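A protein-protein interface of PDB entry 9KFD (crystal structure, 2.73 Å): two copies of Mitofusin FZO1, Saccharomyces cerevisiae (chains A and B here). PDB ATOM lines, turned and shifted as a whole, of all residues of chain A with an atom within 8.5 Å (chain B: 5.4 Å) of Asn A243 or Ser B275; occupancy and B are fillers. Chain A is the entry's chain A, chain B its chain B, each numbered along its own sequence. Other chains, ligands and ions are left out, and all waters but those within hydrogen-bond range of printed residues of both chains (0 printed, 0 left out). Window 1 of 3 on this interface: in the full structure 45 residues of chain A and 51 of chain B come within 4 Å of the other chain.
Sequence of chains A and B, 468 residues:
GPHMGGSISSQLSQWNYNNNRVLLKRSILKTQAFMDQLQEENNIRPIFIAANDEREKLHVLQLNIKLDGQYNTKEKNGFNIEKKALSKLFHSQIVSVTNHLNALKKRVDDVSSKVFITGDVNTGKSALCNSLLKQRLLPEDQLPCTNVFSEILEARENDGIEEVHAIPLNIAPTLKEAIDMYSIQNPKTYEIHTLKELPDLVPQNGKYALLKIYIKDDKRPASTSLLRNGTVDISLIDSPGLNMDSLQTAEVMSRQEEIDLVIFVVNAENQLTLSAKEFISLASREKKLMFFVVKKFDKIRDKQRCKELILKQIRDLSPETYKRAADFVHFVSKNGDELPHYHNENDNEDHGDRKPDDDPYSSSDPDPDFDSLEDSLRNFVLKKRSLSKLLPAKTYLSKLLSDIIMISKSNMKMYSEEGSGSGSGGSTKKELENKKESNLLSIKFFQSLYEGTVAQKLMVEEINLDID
Of the 23 printed residues of chain A, 8 touch a printed residue of chain B. Printed residues of chain A that touch a printed residue of chain B: Tyr A71, Asn A243, Met A244, Asp A245, Ser A246, Thr A273, Leu A274 and Ser A275. Printed residues of chain B that touch a printed residue of chain A: Asp B120, Asn B243, Thr B273, Leu B274, Ser B275, Lys B277 and Glu B278.
Asn A243 touches Asp B120, but with the chains exchanged Asp A120 does not touch Asn B243 (4.7 Å). Asn A243 touches its own counterpart, Asn B243. Asn A243 touches Thr B273, and with the chains exchanged Thr A273 touches Asn B243. Asn A243 touches Ser B275, and with the chains exchanged Ser A275 touches Asn B243. Of the 14 pairs that touch across the chains among the printed residues, 7 have their exchanged pair printed and touching as well.
Among the printed residues, merely in contact across the chains: Asn A243 with Asp B120 (3.9 Å), Asn A243 with Thr B273 (3.3 Å), Met A244 with Thr B273 (3.7 Å), Met A244 with Leu B274 (3.7 Å), Asp A245 with Leu B274 (3.9 Å), Ser A246 with Leu B274 (3.5 Å) and Thr A273 with Asn B243 (3.0 Å).
The side-chain carboxylate of Glu B278 lies within hydrogen-bond range of the side-chain hydroxyl of Tyr A71, at 3.3 Å. ND2 of Asn A243 sits close to ND2 of Asn B243 (3.0 Å). The backbone NH of Leu B274 lies within hydrogen-bond range of the backbone carbonyl oxygen of Asn A243 (3.0 Å). The backbone NH (N) of Ser B275 lies within hydrogen-bond range of the side-chain amide oxygen (OD1) of Asn A243 (2.9 Å). O of Met A244 is in hydrogen-bond range of NZ of Lys B277, at 2.9 Å. The backbone NH of Leu A274 sits at hydrogen-bond distance from the side-chain amide oxygen of Asn B243 (2.9 Å). OD1 of Asn B243 is in hydrogen-bond range of N of Ser A275.
Asn A243 touches just these residues of chain B: Asp B120, Asn B243, Thr B273, Leu B274 and Ser B275. Of the printed residues of chain A, Ser B275 touches Asn A243 (2.9 Å). No residue of chain A comes within 4 Å of Ala B276. Of the printed residues of chain A, Asn B243 touches Asn A243, Thr A273, Leu A274 and Ser A275. Of the printed residues of chain B, Met A244 touches Thr B273 (3.7 Å), Leu B274 (3.7 Å) and Lys B277 (2.9 Å). Printed residues of chain B within 4 Å of Ser A275: Asn B243. Printed residues of chain B within 4 Å of Ser A246: Leu B274. Of the printed residues of chain B, Asp A245 touches Leu B274. Leu B242 touches none of the printed residues of chain A. Asn A270 touches none of the printed residues of chain B. The nearest printed residue of chain B that does not touch Asp A245 is Lys B277 (4.5 Å).
The side-chain carboxylate (OD1) of Asp A120 sits at hydrogen-bond distance from the side-chain hydroxyl (OG) of Ser A275 (2.8 Å). OG1 of Thr A273 sits at hydrogen-bond distance from OG of Ser A275, at 3.3 Å. OG1 of Thr A273 lies close to N of Ala A276. OD1 of Asp B120 is in hydrogen-bond range of OG of Ser B275 (3.0 Å). The side-chain amide nitrogen of Asn B243 sits at hydrogen-bond distance from the side-chain hydroxyl of Ser B275 (3.3 Å). The side-chain hydroxyl (OG) of Ser B275 is in hydrogen-bond range of the side-chain hydroxyl (OG1) of Thr B273 (3.2 Å).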
ATOM      1  N   TYR A  71     -21.979  34.981  29.201  1.00  0.00           N
ATOM      2  CA  TYR A  71     -20.574  34.778  29.531  1.00  0.00           C
ATOM      3  C   TYR A  71     -20.166  35.793  30.588  1.00  0.00           C
ATOM      4  O   TYR A  71     -20.263  37.004  30.360  1.00  0.00           O
ATOM      5  CB  TYR A  71     -19.690  34.906  28.289  1.00  0.00           C
ATOM      6  CG  TYR A  71     -20.018  33.914  27.191  1.00  0.00           C
ATOM      7  CD1 TYR A  71     -21.091  34.126  26.333  1.00  0.00           C
ATOM      8  CD2 TYR A  71     -19.254  32.769  27.015  1.00  0.00           C
ATOM      9  CE1 TYR A  71     -21.391  33.225  25.329  1.00  0.00           C
ATOM     10  CE2 TYR A  71     -19.548  31.861  26.014  1.00  0.00           C
ATOM     11  CZ  TYR A  71     -20.618  32.095  25.174  1.00  0.00           C
ATOM     12  OH  TYR A  71     -20.915  31.196  24.176  1.00  0.00           O
ATOM     13  N   GLY A 119     -11.379  13.630  20.620  1.00  0.00           N
ATOM     14  CA  GLY A 119     -10.630  14.858  20.469  1.00  0.00           C
ATOM     15  C   GLY A 119     -11.416  15.840  19.623  1.00  0.00           C
ATOM     16  O   GLY A 119     -12.568  15.602  19.270  1.00  0.00           O
ATOM     17  N   ASP A 120     -10.765  16.955  19.301  1.00  0.00           N
ATOM     18  CA  ASP A 120     -11.410  17.973  18.487  1.00  0.00           C
ATOM     19  C   ASP A 120     -11.644  17.461  17.070  1.00  0.00           C
ATOM     20  O   ASP A 120     -11.096  16.439  16.645  1.00  0.00           O
ATOM     21  CB  ASP A 120     -10.570  19.249  18.442  1.00  0.00           C
ATOM     22  CG  ASP A 120     -10.836  20.164  19.619  1.00  0.00           C
ATOM     23  OD1 ASP A 120     -11.666  19.807  20.481  1.00  0.00           O
ATOM     24  OD2 ASP A 120     -10.208  21.242  19.683  1.00  0.00           O
ATOM     25  N   VAL A 121     -12.476  18.199  16.332  1.00  0.00           N
ATOM     26  CA  VAL A 121     -12.764  17.839  14.950  1.00  0.00           C
ATOM     27  C   VAL A 121     -11.483  17.869  14.127  1.00  0.00           C
ATOM     28  O   VAL A 121     -10.612  18.731  14.316  1.00  0.00           O
ATOM     29  CB  VAL A 121     -13.828  18.787  14.370  1.00  0.00           C
ATOM     30  CG1 VAL A 121     -13.344  20.231  14.416  1.00  0.00           C
ATOM     31  CG2 VAL A 121     -14.198  18.382  12.948  1.00  0.00           C
ATOM     32  N   ASN A 122     -11.350  16.894  13.223  1.00  0.00           N
ATOM     33  CA  ASN A 122     -10.270  16.855  12.234  1.00  0.00           C
ATOM     34  C   ASN A 122      -8.890  16.766  12.880  1.00  0.00           C
ATOM     35  O   ASN A 122      -7.905  17.264  12.328  1.00  0.00           O
ATOM     36  CB  ASN A 122     -10.335  18.061  11.293  1.00  0.00           C
ATOM     37  CG  ASN A 122     -11.479  17.968  10.306  1.00  0.00           C
ATOM     38  OD1 ASN A 122     -11.911  16.874   9.945  1.00  0.00           O
ATOM     39  ND2 ASN A 122     -11.972  19.116   9.860  1.00  0.00           N
ATOM     40  N   PRO A 144     -15.255  17.619   8.183  1.00  0.00           N
ATOM     41  CA  PRO A 144     -15.888  16.827   9.251  1.00  0.00           C
ATOM     42  C   PRO A 144     -16.529  15.546   8.733  1.00  0.00           C
ATOM     43  O   PRO A 144     -17.343  15.562   7.807  1.00  0.00           O
ATOM     44  CB  PRO A 144     -16.937  17.785   9.829  1.00  0.00           C
ATOM     45  CG  PRO A 144     -16.557  19.164   9.353  1.00  0.00           C
ATOM     46  CD  PRO A 144     -15.386  19.067   8.422  1.00  0.00           C
ATOM     47  N   PRO A 240     -17.085  11.014  17.429  1.00  0.00           N
ATOM     48  CA  PRO A 240     -17.286  12.269  16.699  1.00  0.00           C
ATOM     49  C   PRO A 240     -16.424  13.375  17.284  1.00  0.00           C
ATOM     50  O   PRO A 240     -15.948  13.300  18.419  1.00  0.00           O
ATOM     51  CB  PRO A 240     -18.779  12.563  16.890  1.00  0.00           C
ATOM     52  CG  PRO A 240     -19.391  11.240  17.189  1.00  0.00           C
ATOM     53  CD  PRO A 240     -18.348  10.481  17.963  1.00  0.00           C
ATOM     54  N   GLY A 241     -16.223  14.421  16.488  1.00  0.00           N
ATOM     55  CA  GLY A 241     -15.350  15.497  16.906  1.00  0.00           C
ATOM     56  C   GLY A 241     -15.987  16.383  17.959  1.00  0.00           C
ATOM     57  O   GLY A 241     -17.204  16.556  18.017  1.00  0.00           O
ATOM     58  N   LEU A 242     -15.138  16.940  18.817  1.00  0.00           N
ATOM     59  CA  LEU A 242     -15.557  18.002  19.712  1.00  0.00           C
ATOM     60  C   LEU A 242     -15.599  19.329  18.956  1.00  0.00           C
ATOM     61  O   LEU A 242     -15.075  19.459  17.845  1.00  0.00           O
ATOM     62  CB  LEU A 242     -14.615  18.096  20.912  1.00  0.00           C
ATOM     63  CG  LEU A 242     -14.560  16.900  21.868  1.00  0.00           C
ATOM     64  CD1 LEU A 242     -13.410  17.054  22.851  1.00  0.00           C
ATOM     65  CD2 LEU A 242     -15.877  16.742  22.612  1.00  0.00           C
ATOM     66  N   ASN A 243     -16.244  20.321  19.570  1.00  0.00           N
ATOM     67  CA  ASN A 243     -16.334  21.674  19.015  1.00  0.00           C
ATOM     68  C   ASN A 243     -17.050  21.686  17.666  1.00  0.00           C
ATOM     69  O   ASN A 243     -16.641  22.376  16.731  1.00  0.00           O
ATOM     70  CB  ASN A 243     -14.951  22.321  18.898  1.00  0.00           C
ATOM     71  CG  ASN A 243     -15.021  23.833  18.815  1.00  0.00           C
ATOM     72  OD1 ASN A 243     -15.970  24.448  19.303  1.00  0.00           O
ATOM     73  ND2 ASN A 243     -14.020  24.440  18.187  1.00  0.00           N
ATOM     74  N   MET A 244     -18.134  20.925  17.565  1.00  0.00           N
ATOM     75  CA  MET A 244     -18.925  20.884  16.340  1.00  0.00           C
ATOM     76  C   MET A 244     -20.382  21.218  16.625  1.00  0.00           C
ATOM     77  O   MET A 244     -20.925  22.198  16.115  1.00  0.00           O
ATOM     78  CB  MET A 244     -18.820  19.509  15.681  1.00  0.00           C
ATOM     79  CG  MET A 244     -17.593  19.342  14.806  1.00  0.00           C
ATOM     80  SD  MET A 244     -17.808  20.204  13.068  1.00  0.00           S
ATOM     81  CE  MET A 244     -16.468  21.601  13.274  1.00  0.00           C
ATOM     82  N   ASP A 245     -21.007  20.386  17.450  1.00  0.00           N
ATOM     83  CA  ASP A 245     -22.396  20.541  17.844  1.00  0.00           C
ATOM     84  C   ASP A 245     -22.476  20.475  19.361  1.00  0.00           C
ATOM     85  O   ASP A 245     -21.683  19.786  20.008  1.00  0.00           O
ATOM     86  CB  ASP A 245     -23.272  19.449  17.201  1.00  0.00           C
ATOM     87  CG  ASP A 245     -24.754  19.614  17.505  1.00  0.00           C
ATOM     88  OD1 ASP A 245     -25.130  20.549  18.247  1.00  0.00           O
ATOM     89  OD2 ASP A 245     -25.551  18.794  16.997  1.00  0.00           O
ATOM     90  N   SER A 246     -23.434  21.211  19.925  1.00  0.00           N
ATOM     91  CA  SER A 246     -23.614  21.187  21.372  1.00  0.00           C
ATOM     92  C   SER A 246     -24.071  19.814  21.846  1.00  0.00           C
ATOM     93  O   SER A 246     -23.578  19.304  22.860  1.00  0.00           O
ATOM     94  CB  SER A 246     -24.612  22.263  21.797  1.00  0.00           C
ATOM     95  OG  SER A 246     -25.909  21.717  21.954  1.00  0.00           O
ATOM     96  N   GLN A 248     -23.631  16.964  20.137  1.00  0.00           N
ATOM     97  CA  GLN A 248     -22.542  16.037  19.842  1.00  0.00           C
ATOM     98  C   GLN A 248     -21.509  16.026  20.961  1.00  0.00           C
ATOM     99  O   GLN A 248     -21.031  14.959  21.363  1.00  0.00           O
ATOM    100  CB  GLN A 248     -21.891  16.407  18.512  1.00  0.00           C
ATOM    101  CG  GLN A 248     -20.735  15.518  18.105  1.00  0.00           C
ATOM    102  CD  GLN A 248     -20.529  15.500  16.605  1.00  0.00           C
ATOM    103  OE1 GLN A 248     -21.453  15.210  15.844  1.00  0.00           O
ATOM    104  NE2 GLN A 248     -19.314  15.818  16.168  1.00  0.00           N
ATOM    105  N   THR A 249     -21.152  17.204  21.476  1.00  0.00           N
ATOM    106  CA  THR A 249     -20.242  17.261  22.614  1.00  0.00           C
ATOM    107  C   THR A 249     -20.837  16.549  23.822  1.00  0.00           C
ATOM    108  O   THR A 249     -20.148  15.773  24.495  1.00  0.00           O
ATOM    109  CB  THR A 249     -19.912  18.716  22.955  1.00  0.00           C
ATOM    110  OG1 THR A 249     -19.077  19.273  21.932  1.00  0.00           O
ATOM    111  CG2 THR A 249     -19.184  18.802  24.292  1.00  0.00           C
ATOM    112  N   ALA A 250     -22.124  16.779  24.094  1.00  0.00           N
ATOM    113  CA  ALA A 250     -22.774  16.134  25.231  1.00  0.00           C
ATOM    114  C   ALA A 250     -22.740  14.616  25.106  1.00  0.00           C
ATOM    115  O   ALA A 250     -22.498  13.912  26.094  1.00  0.00           O
ATOM    116  CB  ALA A 250     -24.215  16.628  25.360  1.00  0.00           C
ATOM    117  N   VAL A 252     -20.505  12.863  23.501  1.00  0.00           N
ATOM    118  CA  VAL A 252     -19.128  12.440  23.732  1.00  0.00           C
ATOM    119  C   VAL A 252     -18.811  12.461  25.222  1.00  0.00           C
ATOM    120  O   VAL A 252     -18.106  11.581  25.732  1.00  0.00           O
ATOM    121  CB  VAL A 252     -18.159  13.321  22.923  1.00  0.00           C
ATOM    122  CG1 VAL A 252     -16.722  13.092  23.366  1.00  0.00           C
ATOM    123  CG2 VAL A 252     -18.311  13.044  21.436  1.00  0.00           C
ATOM    124  N   ASN A 270      -3.026  23.778  17.239  1.00  0.00           N
ATOM    125  CA  ASN A 270      -3.928  24.391  18.204  1.00  0.00           C
ATOM    126  C   ASN A 270      -3.600  24.031  19.643  1.00  0.00           C
ATOM    127  O   ASN A 270      -4.098  24.699  20.556  1.00  0.00           O
ATOM    128  CB  ASN A 270      -5.371  23.987  17.903  1.00  0.00           C
ATOM    129  CG  ASN A 270      -5.929  24.684  16.684  1.00  0.00           C
ATOM    130  OD1 ASN A 270      -5.284  25.559  16.105  1.00  0.00           O
ATOM    131  ND2 ASN A 270      -7.140  24.303  16.286  1.00  0.00           N
ATOM    132  N   THR A 273      -7.115  22.758  22.989  1.00  0.00           N
ATOM    133  CA  THR A 273      -8.107  23.803  22.826  1.00  0.00           C
ATOM    134  C   THR A 273      -9.064  23.818  24.018  1.00  0.00           C
ATOM    135  O   THR A 273      -9.065  22.915  24.860  1.00  0.00           O
ATOM    136  CB  THR A 273      -8.876  23.604  21.523  1.00  0.00           C
ATOM    137  OG1 THR A 273      -9.448  22.291  21.498  1.00  0.00           O
ATOM    138  CG2 THR A 273      -7.954  23.775  20.328  1.00  0.00           C
ATOM    139  N   LEU A 274      -9.887  24.867  24.084  1.00  0.00           N
ATOM    140  CA  LEU A 274     -10.831  24.999  25.189  1.00  0.00           C
ATOM    141  C   LEU A 274     -11.831  23.851  25.196  1.00  0.00           C
ATOM    142  O   LEU A 274     -12.104  23.258  26.246  1.00  0.00           O
ATOM    143  CB  LEU A 274     -11.558  26.342  25.113  1.00  0.00           C
ATOM    144  CG  LEU A 274     -12.671  26.507  26.152  1.00  0.00           C
ATOM    145  CD1 LEU A 274     -12.130  27.146  27.418  1.00  0.00           C
ATOM    146  CD2 LEU A 274     -13.832  27.314  25.594  1.00  0.00           C
ATOM    147  N   SER A 275     -12.395  23.528  24.028  1.00  0.00           N
ATOM    148  CA  SER A 275     -13.282  22.373  23.933  1.00  0.00           C
ATOM    149  C   SER A 275     -12.572  21.097  24.356  1.00  0.00           C
ATOM    150  O   SER A 275     -13.201  20.190  24.913  1.00  0.00           O
ATOM    151  CB  SER A 275     -13.814  22.233  22.507  1.00  0.00           C
ATOM    152  OG  SER A 275     -12.753  22.203  21.569  1.00  0.00           O
ATOM    153  N   ALA A 276     -11.263  21.012  24.105  1.00  0.00           N
ATOM    154  CA  ALA A 276     -10.492  19.851  24.535  1.00  0.00           C
ATOM    155  C   ALA A 276     -10.276  19.863  26.043  1.00  0.00           C
ATOM    156  O   ALA A 276     -10.373  18.818  26.698  1.00  0.00           O
ATOM    157  CB  ALA A 276      -9.154  19.813  23.798  1.00  0.00           C
ATOM    158  N   GLU A 278     -12.243  21.190  28.212  1.00  0.00           N
ATOM    159  CA  GLU A 278     -13.523  20.888  28.842  1.00  0.00           C
ATOM    160  C   GLU A 278     -13.762  19.387  28.935  1.00  0.00           C
ATOM    161  O   GLU A 278     -14.362  18.914  29.907  1.00  0.00           O
ATOM    162  CB  GLU A 278     -14.655  21.568  28.072  1.00  0.00           C
ATOM    163  CG  GLU A 278     -14.717  23.076  28.277  1.00  0.00           C
ATOM    164  CD  GLU A 278     -15.858  23.727  27.516  1.00  0.00           C
ATOM    165  OE1 GLU A 278     -16.469  23.047  26.661  1.00  0.00           O
ATOM    166  OE2 GLU A 278     -16.147  24.917  27.776  1.00  0.00           O
ATOM    167  N   ASP B 120     -11.891  31.651  15.423  1.00  0.00           N
ATOM    168  CA  ASP B 120     -11.196  30.617  16.173  1.00  0.00           C
ATOM    169  C   ASP B 120      -9.690  30.860  16.156  1.00  0.00           C
ATOM    170  O   ASP B 120      -9.160  31.624  15.345  1.00  0.00           O
ATOM    171  CB  ASP B 120     -11.504  29.232  15.600  1.00  0.00           C
ATOM    172  CG  ASP B 120     -12.747  28.615  16.207  1.00  0.00           C
ATOM    173  OD1 ASP B 120     -13.406  29.284  17.029  1.00  0.00           O
ATOM    174  OD2 ASP B 120     -13.062  27.455  15.866  1.00  0.00           O
ATOM    175  N   LEU B 242     -10.900  32.583  19.576  1.00  0.00           N
ATOM    176  CA  LEU B 242     -11.887  31.841  20.340  1.00  0.00           C
ATOM    177  C   LEU B 242     -11.397  30.417  20.584  1.00  0.00           C
ATOM    178  O   LEU B 242     -10.469  29.928  19.932  1.00  0.00           O
ATOM    179  CB  LEU B 242     -13.230  31.813  19.608  1.00  0.00           C
ATOM    180  CG  LEU B 242     -14.080  33.086  19.616  1.00  0.00           C
ATOM    181  CD1 LEU B 242     -15.127  33.040  18.512  1.00  0.00           C
ATOM    182  CD2 LEU B 242     -14.739  33.278  20.974  1.00  0.00           C
ATOM    183  N   ASN B 243     -12.035  29.755  21.548  1.00  0.00           N
ATOM    184  CA  ASN B 243     -11.762  28.357  21.883  1.00  0.00           C
ATOM    185  C   ASN B 243     -10.303  28.176  22.311  1.00  0.00           C
ATOM    186  O   ASN B 243      -9.523  27.451  21.691  1.00  0.00           O
ATOM    187  CB  ASN B 243     -12.126  27.440  20.709  1.00  0.00           C
ATOM    188  CG  ASN B 243     -12.213  25.984  21.111  1.00  0.00           C
ATOM    189  OD1 ASN B 243     -11.247  25.400  21.579  1.00  0.00           O
ATOM    190  ND2 ASN B 243     -13.385  25.392  20.932  1.00  0.00           N
ATOM    191  N   PHE B 264     -15.650  37.878  10.568  1.00  0.00           N
ATOM    192  CA  PHE B 264     -15.410  36.561  11.143  1.00  0.00           C
ATOM    193  C   PHE B 264     -14.524  35.750  10.207  1.00  0.00           C
ATOM    194  O   PHE B 264     -14.870  35.543   9.039  1.00  0.00           O
ATOM    195  CB  PHE B 264     -16.722  35.828  11.406  1.00  0.00           C
ATOM    196  CG  PHE B 264     -16.608  34.757  12.447  1.00  0.00           C
ATOM    197  CD1 PHE B 264     -16.722  35.068  13.792  1.00  0.00           C
ATOM    198  CD2 PHE B 264     -16.359  33.443  12.084  1.00  0.00           C
ATOM    199  CE1 PHE B 264     -16.606  34.085  14.755  1.00  0.00           C
ATOM    200  CE2 PHE B 264     -16.241  32.457  13.042  1.00  0.00           C
ATOM    201  CZ  PHE B 264     -16.363  32.780  14.378  1.00  0.00           C
ATOM    202  N   THR B 273     -17.105  26.149  13.575  1.00  0.00           N
ATOM    203  CA  THR B 273     -17.098  25.276  14.738  1.00  0.00           C
ATOM    204  C   THR B 273     -18.181  25.705  15.729  1.00  0.00           C
ATOM    205  O   THR B 273     -18.864  26.718  15.550  1.00  0.00           O
ATOM    206  CB  THR B 273     -15.728  25.299  15.414  1.00  0.00           C
ATOM    207  OG1 THR B 273     -15.296  26.657  15.571  1.00  0.00           O
ATOM    208  CG2 THR B 273     -14.707  24.546  14.573  1.00  0.00           C
ATOM    209  N   LEU B 274     -18.334  24.911  16.792  1.00  0.00           N
ATOM    210  CA  LEU B 274     -19.292  25.261  17.837  1.00  0.00           C
ATOM    211  C   LEU B 274     -18.918  26.585  18.490  1.00  0.00           C
ATOM    212  O   LEU B 274     -19.770  27.466  18.666  1.00  0.00           O
ATOM    213  CB  LEU B 274     -19.370  24.151  18.883  1.00  0.00           C
ATOM    214  CG  LEU B 274     -20.162  24.528  20.139  1.00  0.00           C
ATOM    215  CD1 LEU B 274     -21.642  24.224  19.955  1.00  0.00           C
ATOM    216  CD2 LEU B 274     -19.613  23.815  21.364  1.00  0.00           C
ATOM    217  N   SER B 275     -17.641  26.745  18.850  1.00  0.00           N
ATOM    218  CA  SER B 275     -17.176  28.018  19.391  1.00  0.00           C
ATOM    219  C   SER B 275     -17.432  29.163  18.421  1.00  0.00           C
ATOM    220  O   SER B 275     -17.717  30.286  18.850  1.00  0.00           O
ATOM    221  CB  SER B 275     -15.687  27.929  19.731  1.00  0.00           C
ATOM    222  OG  SER B 275     -14.961  27.306  18.686  1.00  0.00           O
ATOM    223  N   ALA B 276     -17.348  28.895  17.116  1.00  0.00           N
ATOM    224  CA  ALA B 276     -17.659  29.918  16.123  1.00  0.00           C
ATOM    225  C   ALA B 276     -19.147  30.248  16.123  1.00  0.00           C
ATOM    226  O   ALA B 276     -19.534  31.424  16.166  1.00  0.00           O
ATOM    227  CB  ALA B 276     -17.209  29.454  14.738  1.00  0.00           C
ATOM    228  N   LYS B 277     -19.998  29.218  16.073  1.00  0.00           N
ATOM    229  CA  LYS B 277     -21.441  29.436  16.112  1.00  0.00           C
ATOM    230  C   LYS B 277     -21.867  30.197  17.362  1.00  0.00           C
ATOM    231  O   LYS B 277     -22.845  30.952  17.325  1.00  0.00           O
ATOM    232  CB  LYS B 277     -22.179  28.098  16.047  1.00  0.00           C
ATOM    233  CG  LYS B 277     -22.107  27.384  14.712  1.00  0.00           C
ATOM    234  CD  LYS B 277     -23.152  26.280  14.641  1.00  0.00           C
ATOM    235  CE  LYS B 277     -22.585  25.018  14.015  1.00  0.00           C
ATOM    236  NZ  LYS B 277     -22.991  23.796  14.770  1.00  0.00           N
ATOM    237  N   GLU B 278     -21.150  30.013  18.474  1.00  0.00           N
ATOM    238  CA  GLU B 278     -21.539  30.680  19.713  1.00  0.00           C
ATOM    239  C   GLU B 278     -21.257  32.179  19.655  1.00  0.00           C
ATOM    240  O   GLU B 278     -22.012  32.975  20.225  1.00  0.00           O
ATOM    241  CB  GLU B 278     -20.836  30.029  20.905  1.00  0.00           C
ATOM    242  CG  GLU B 278     -21.327  28.615  21.194  1.00  0.00           C
ATOM    243  CD  GLU B 278     -20.666  27.990  22.409  1.00  0.00           C
ATOM    244  OE1 GLU B 278     -19.586  28.467  22.816  1.00  0.00           O
ATOM    245  OE2 GLU B 278     -21.232  27.021  22.959  1.00  0.00           O
ATOM    246  N   PHE B 279     -20.182  32.587  18.974  1.00  0.00           N
ATOM    247  CA  PHE B 279     -19.981  34.008  18.706  1.00  0.00           C
ATOM    248  C   PHE B 279     -21.082  34.542  17.798  1.00  0.00           C
ATOM    249  O   PHE B 279     -21.787  35.497  18.144  1.00  0.00           O
ATOM    250  CB  PHE B 279     -18.604  34.251  18.071  1.00  0.00           C
ATOM    251  CG  PHE B 279     -18.276  35.718  17.846  1.00  0.00           C
ATOM    252  CD1 PHE B 279     -18.901  36.450  16.846  1.00  0.00           C
ATOM    253  CD2 PHE B 279     -17.330  36.357  18.628  1.00  0.00           C
ATOM    254  CE1 PHE B 279     -18.602  37.786  16.650  1.00  0.00           C
ATOM    255  CE2 PHE B 279     -17.023  37.691  18.433  1.00  0.00           C
ATOM    256  CZ  PHE B 279     -17.661  38.406  17.444  1.00  0.00           C
